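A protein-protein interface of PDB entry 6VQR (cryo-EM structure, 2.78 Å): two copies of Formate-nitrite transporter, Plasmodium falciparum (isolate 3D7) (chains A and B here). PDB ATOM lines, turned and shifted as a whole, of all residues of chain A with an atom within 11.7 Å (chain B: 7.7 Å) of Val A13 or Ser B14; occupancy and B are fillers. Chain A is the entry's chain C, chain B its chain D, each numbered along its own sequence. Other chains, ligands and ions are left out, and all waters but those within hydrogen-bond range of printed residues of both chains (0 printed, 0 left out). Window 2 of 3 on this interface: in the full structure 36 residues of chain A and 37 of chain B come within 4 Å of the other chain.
The backbone carbonyl oxygen (O) of Val A13 lies within hydrogen-bond range of the backbone NH (N) of Lys B16 (2.9 Å).
The backbone NH (N) of Ile A15 sits at hydrogen-bond distance from the backbone carbonyl oxygen (O) of Lys B16, at 2.7 Å.
Among the printed residues, merely in contact across the chains: Pro A12 with Ser B14 (3.9 Å), Pro A12 with Ile B15 (3.9 Å), Pro A12 with Lys B16 (3.7 Å), Val A13 with Ser B14 (3.5 Å), Val A13 with Ile B15 (3.4 Å), Ser A14 with Lys B16 (3.6 Å), Ile A15 with Ile B15 (3.5 Å) and Ile A15 with Ser B17 (3.5 Å).
Of the printed residues of chain B, Pro A12 touches Ser B14 (3.9 Å), Ile B15 (3.9 Å) and Lys B16 (3.7 Å).
Of the printed residues of chain B, Val A13 touches Ser B14, Ile B15 and Lys B16.
Printed residues of chain B within 4 Å of Ser A14: Lys B16.
Lys A16 touches none of the printed residues of chain B.
Val B13 touches none of the printed residues of chain A.
Of chain A, only Pro A12 and Val A13 come within 4 Å of Ser B14.
Of chain A, only Pro A12, Val A13 and Ile A15 come within 4 Å of Ile B15.
Lys B16 touches just these residues of chain A: Pro A12 (3.7 Å), Val A13 (2.9 Å), Ser A14 (3.6 Å) and Ile A15 (2.7 Å).
Of the printed residues of chain A, Ser B17 touches Ile A15.
Of the 9 printed residues of chain B, 4 touch a printed residue of chain A.
Printed residues of chain B that touch a printed residue of chain A: Ser B14, Ile B15, Lys B16 and Ser B17.
Hydrophobic or aromatic side chains of chain B that line the printed part of chain A: Ile B15.
Of the 9 printed residues of chain A, 4 touch a printed residue of chain B.
Among the printed residues, 10 pairs touch across the chains.
Among the printed residues, no Asp or Glu carboxylate lies within 4 Å of a Lys or Arg side-chain nitrogen of the other chain.
Pro A12 touches Ser B14, but with the chains exchanged Ser A14 does not touch Pro B12 (12.9 Å).
Pro A12 touches Lys B16, but with the chains exchanged Lys A16 does not touch Pro B12 (15.8 Å).
Val A13 touches Ser B14, but with the chains exchanged Ser A14 does not touch Val B13 (9.0 Å).
Ser A14 touches Lys B16, but with the chains exchanged Lys A16 does not touch Ser B14 (10.3 Å).
7 positions are printed for both chains.
Of the 10 pairs that touch across the chains among the printed residues, 1 has its exchanged pair printed and touching as well.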
ATOM      1  N   VAL A   9      12.490 -20.656   0.214  1.00  0.00           N
ATOM      2  CA  VAL A   9      13.540 -21.333  -0.535  1.00  0.00           C
ATOM      3  C   VAL A   9      14.618 -20.336  -0.945  1.00  0.00           C
ATOM      4  O   VAL A   9      14.381 -19.128  -0.965  1.00  0.00           O
ATOM      5  CB  VAL A   9      12.970 -22.058  -1.764  1.00  0.00           C
ATOM      6  CG1 VAL A   9      12.400 -23.407  -1.363  1.00  0.00           C
ATOM      7  CG2 VAL A   9      11.909 -21.202  -2.437  1.00  0.00           C
ATOM      8  N   LEU A  10      15.801 -20.847  -1.274  1.00  0.00           N
ATOM      9  CA  LEU A  10      16.927 -19.979  -1.581  1.00  0.00           C
ATOM     10  C   LEU A  10      16.689 -19.241  -2.889  1.00  0.00           C
ATOM     11  O   LEU A  10      16.337 -19.850  -3.904  1.00  0.00           O
ATOM     12  CB  LEU A  10      18.220 -20.790  -1.652  1.00  0.00           C
ATOM     13  CG  LEU A  10      18.334 -21.916  -2.684  1.00  0.00           C
ATOM     14  CD1 LEU A  10      19.234 -21.502  -3.841  1.00  0.00           C
ATOM     15  CD2 LEU A  10      18.843 -23.196  -2.034  1.00  0.00           C
ATOM     16  N   ASP A  11      16.864 -17.921  -2.860  1.00  0.00           N
ATOM     17  CA  ASP A  11      16.773 -17.103  -4.063  1.00  0.00           C
ATOM     18  C   ASP A  11      17.438 -15.744  -3.868  1.00  0.00           C
ATOM     19  O   ASP A  11      16.757 -14.714  -3.839  1.00  0.00           O
ATOM     20  CB  ASP A  11      15.307 -16.955  -4.497  1.00  0.00           C
ATOM     21  CG  ASP A  11      14.443 -16.248  -3.462  1.00  0.00           C
ATOM     22  OD1 ASP A  11      14.887 -16.103  -2.303  1.00  0.00           O
ATOM     23  OD2 ASP A  11      13.317 -15.840  -3.813  1.00  0.00           O
ATOM     24  N   PRO A  12      18.764 -15.694  -3.752  1.00  0.00           N
ATOM     25  CA  PRO A  12      19.444 -14.403  -3.618  1.00  0.00           C
ATOM     26  C   PRO A  12      19.260 -13.543  -4.859  1.00  0.00           C
ATOM     27  O   PRO A  12      18.758 -13.982  -5.895  1.00  0.00           O
ATOM     28  CB  PRO A  12      20.909 -14.795  -3.412  1.00  0.00           C
ATOM     29  CG  PRO A  12      21.020 -16.157  -3.957  1.00  0.00           C
ATOM     30  CD  PRO A  12      19.711 -16.816  -3.699  1.00  0.00           C
ATOM     31  N   VAL A  13      19.670 -12.287  -4.742  1.00  0.00           N
ATOM     32  CA  VAL A  13      19.535 -11.312  -5.816  1.00  0.00           C
ATOM     33  C   VAL A  13      20.865 -11.197  -6.538  1.00  0.00           C
ATOM     34  O   VAL A  13      21.914 -11.043  -5.901  1.00  0.00           O
ATOM     35  CB  VAL A  13      19.084  -9.947  -5.276  1.00  0.00           C
ATOM     36  CG1 VAL A  13      18.602  -9.064  -6.414  1.00  0.00           C
ATOM     37  CG2 VAL A  13      17.995 -10.125  -4.231  1.00  0.00           C
ATOM     38  N   SER A  14      20.826 -11.275  -7.863  1.00  0.00           N
ATOM     39  CA  SER A  14      22.038 -11.192  -8.667  1.00  0.00           C
ATOM     40  C   SER A  14      22.544  -9.760  -8.660  1.00  0.00           C
ATOM     41  O   SER A  14      21.984  -8.894  -9.337  1.00  0.00           O
ATOM     42  CB  SER A  14      21.756 -11.663 -10.087  1.00  0.00           C
ATOM     43  OG  SER A  14      20.515 -11.159 -10.540  1.00  0.00           O
ATOM     44  N   ILE A  15      23.602  -9.510  -7.900  1.00  0.00           N
ATOM     45  CA  ILE A  15      24.149  -8.176  -7.739  1.00  0.00           C
ATOM     46  C   ILE A  15      25.265  -7.971  -8.753  1.00  0.00           C
ATOM     47  O   ILE A  15      25.842  -8.918  -9.287  1.00  0.00           O
ATOM     48  CB  ILE A  15      24.660  -7.947  -6.300  1.00  0.00           C
ATOM     49  CG1 ILE A  15      24.660  -6.465  -5.945  1.00  0.00           C
ATOM     50  CG2 ILE A  15      26.057  -8.485  -6.138  1.00  0.00           C
ATOM     51  CD1 ILE A  15      25.440  -6.169  -4.685  1.00  0.00           C
ATOM     52  N   LYS A  16      25.568  -6.704  -9.029  1.00  0.00           N
ATOM     53  CA  LYS A  16      26.677  -6.359  -9.913  1.00  0.00           C
ATOM     54  C   LYS A  16      27.265  -5.052  -9.395  1.00  0.00           C
ATOM     55  O   LYS A  16      26.721  -3.978  -9.657  1.00  0.00           O
ATOM     56  CB  LYS A  16      26.212  -6.243 -11.355  1.00  0.00           C
ATOM     57  CG  LYS A  16      27.212  -5.614 -12.294  1.00  0.00           C
ATOM     58  CD  LYS A  16      26.760  -5.762 -13.732  1.00  0.00           C
ATOM     59  CE  LYS A  16      26.564  -4.413 -14.385  1.00  0.00           C
ATOM     60  NZ  LYS A  16      25.587  -3.575 -13.638  1.00  0.00           N
ATOM     61  N   SER A  17      28.362  -5.155  -8.649  1.00  0.00           N
ATOM     62  CA  SER A  17      28.950  -3.989  -8.005  1.00  0.00           C
ATOM     63  C   SER A  17      29.733  -3.104  -8.962  1.00  0.00           C
ATOM     64  O   SER A  17      30.104  -1.988  -8.585  1.00  0.00           O
ATOM     65  CB  SER A  17      29.871  -4.420  -6.867  1.00  0.00           C
ATOM     66  OG  SER A  17      30.964  -3.529  -6.759  1.00  0.00           O
ATOM     67  N   ASP B  11      15.362  -7.449   9.365  1.00  0.00           N
ATOM     68  CA  ASP B  11      15.877  -8.545   8.555  1.00  0.00           C
ATOM     69  C   ASP B  11      16.407  -8.023   7.225  1.00  0.00           C
ATOM     70  O   ASP B  11      15.719  -7.251   6.550  1.00  0.00           O
ATOM     71  CB  ASP B  11      14.784  -9.585   8.318  1.00  0.00           C
ATOM     72  CG  ASP B  11      13.436  -8.956   8.014  1.00  0.00           C
ATOM     73  OD1 ASP B  11      13.079  -7.959   8.676  1.00  0.00           O
ATOM     74  OD2 ASP B  11      12.731  -9.462   7.115  1.00  0.00           O
ATOM     75  N   PRO B  12      17.612  -8.408   6.820  1.00  0.00           N
ATOM     76  CA  PRO B  12      18.124  -7.978   5.518  1.00  0.00           C
ATOM     77  C   PRO B  12      17.576  -8.835   4.395  1.00  0.00           C
ATOM     78  O   PRO B  12      16.685  -9.660   4.619  1.00  0.00           O
ATOM     79  CB  PRO B  12      19.636  -8.148   5.668  1.00  0.00           C
ATOM     80  CG  PRO B  12      19.773  -9.243   6.627  1.00  0.00           C
ATOM     81  CD  PRO B  12      18.618  -9.158   7.581  1.00  0.00           C
ATOM     82  N   VAL B  13      18.083  -8.639   3.182  1.00  0.00           N
ATOM     83  CA  VAL B  13      17.735  -9.471   2.041  1.00  0.00           C
ATOM     84  C   VAL B  13      19.018 -10.041   1.463  1.00  0.00           C
ATOM     85  O   VAL B  13      20.042  -9.352   1.404  1.00  0.00           O
ATOM     86  CB  VAL B  13      16.946  -8.682   0.979  1.00  0.00           C
ATOM     87  CG1 VAL B  13      17.748  -7.491   0.489  1.00  0.00           C
ATOM     88  CG2 VAL B  13      16.548  -9.591  -0.174  1.00  0.00           C
ATOM     89  N   SER B  14      18.969 -11.308   1.060  1.00  0.00           N
ATOM     90  CA  SER B  14      20.161 -11.981   0.572  1.00  0.00           C
ATOM     91  C   SER B  14      20.615 -11.364  -0.746  1.00  0.00           C
ATOM     92  O   SER B  14      19.903 -10.581  -1.377  1.00  0.00           O
ATOM     93  CB  SER B  14      19.898 -13.474   0.402  1.00  0.00           C
ATOM     94  OG  SER B  14      21.107 -14.209   0.457  1.00  0.00           O
ATOM     95  N   ILE B  15      21.825 -11.727  -1.165  1.00  0.00           N
ATOM     96  CA  ILE B  15      22.411 -11.154  -2.366  1.00  0.00           C
ATOM     97  C   ILE B  15      23.578 -12.035  -2.781  1.00  0.00           C
ATOM     98  O   ILE B  15      24.162 -12.742  -1.956  1.00  0.00           O
ATOM     99  CB  ILE B  15      22.834  -9.686  -2.118  1.00  0.00           C
ATOM    100  CG1 ILE B  15      22.707  -8.869  -3.392  1.00  0.00           C
ATOM    101  CG2 ILE B  15      24.253  -9.610  -1.611  1.00  0.00           C
ATOM    102  CD1 ILE B  15      22.566  -7.395  -3.126  1.00  0.00           C
ATOM    103  N   LYS B  16      23.898 -12.018  -4.073  1.00  0.00           N
ATOM    104  CA  LYS B  16      24.978 -12.837  -4.604  1.00  0.00           C
ATOM    105  C   LYS B  16      25.584 -12.134  -5.804  1.00  0.00           C
ATOM    106  O   LYS B  16      24.884 -11.442  -6.545  1.00  0.00           O
ATOM    107  CB  LYS B  16      24.489 -14.233  -5.002  1.00  0.00           C
ATOM    108  CG  LYS B  16      23.744 -14.282  -6.325  1.00  0.00           C
ATOM    109  CD  LYS B  16      23.424 -15.710  -6.736  1.00  0.00           C
ATOM    110  CE  LYS B  16      22.807 -15.765  -8.126  1.00  0.00           C
ATOM    111  NZ  LYS B  16      21.505 -15.049  -8.196  1.00  0.00           N
ATOM    112  N   SER B  17      26.891 -12.311  -5.987  1.00  0.00           N
ATOM    113  CA  SER B  17      27.609 -11.693  -7.090  1.00  0.00           C
ATOM    114  C   SER B  17      28.296 -12.681  -8.007  1.00  0.00           C
ATOM    115  O   SER B  17      28.610 -12.320  -9.143  1.00  0.00           O
ATOM    116  CB  SER B  17      28.676 -10.722  -6.571  1.00  0.00           C
ATOM    117  OG  SER B  17      29.704 -10.568  -7.531  1.00  0.00           O
ATOM    118  N   VAL B  18      28.558 -13.899  -7.549  1.00  0.00           N
ATOM    119  CA  VAL B  18      29.222 -14.907  -8.385  1.00  0.00           C
ATOM    120  C   VAL B  18      28.110 -15.668  -9.095  1.00  0.00           C
ATOM    121  O   VAL B  18      27.681 -16.755  -8.698  1.00  0.00           O
ATOM    122  CB  VAL B  18      30.144 -15.807  -7.568  1.00  0.00           C
ATOM    123  CG1 VAL B  18      31.411 -15.051  -7.238  1.00  0.00           C
ATOM    124  CG2 VAL B  18      29.447 -16.216  -6.290  1.00  0.00           C
ATOM    125  N   CYS B  19      27.634 -15.081 -10.183  1.00  0.00           N
ATOM    126  CA  CYS B  19      26.621 -15.681 -11.038  1.00  0.00           C
ATOM    127  C   CYS B  19      27.367 -16.103 -12.301  1.00  0.00           C
ATOM    128  O   CYS B  19      27.497 -15.331 -13.253  1.00  0.00           O
ATOM    129  CB  CYS B  19      25.481 -14.695 -11.305  1.00  0.00           C
ATOM    130  SG  CYS B  19      24.488 -14.990 -12.776  1.00  0.00           S
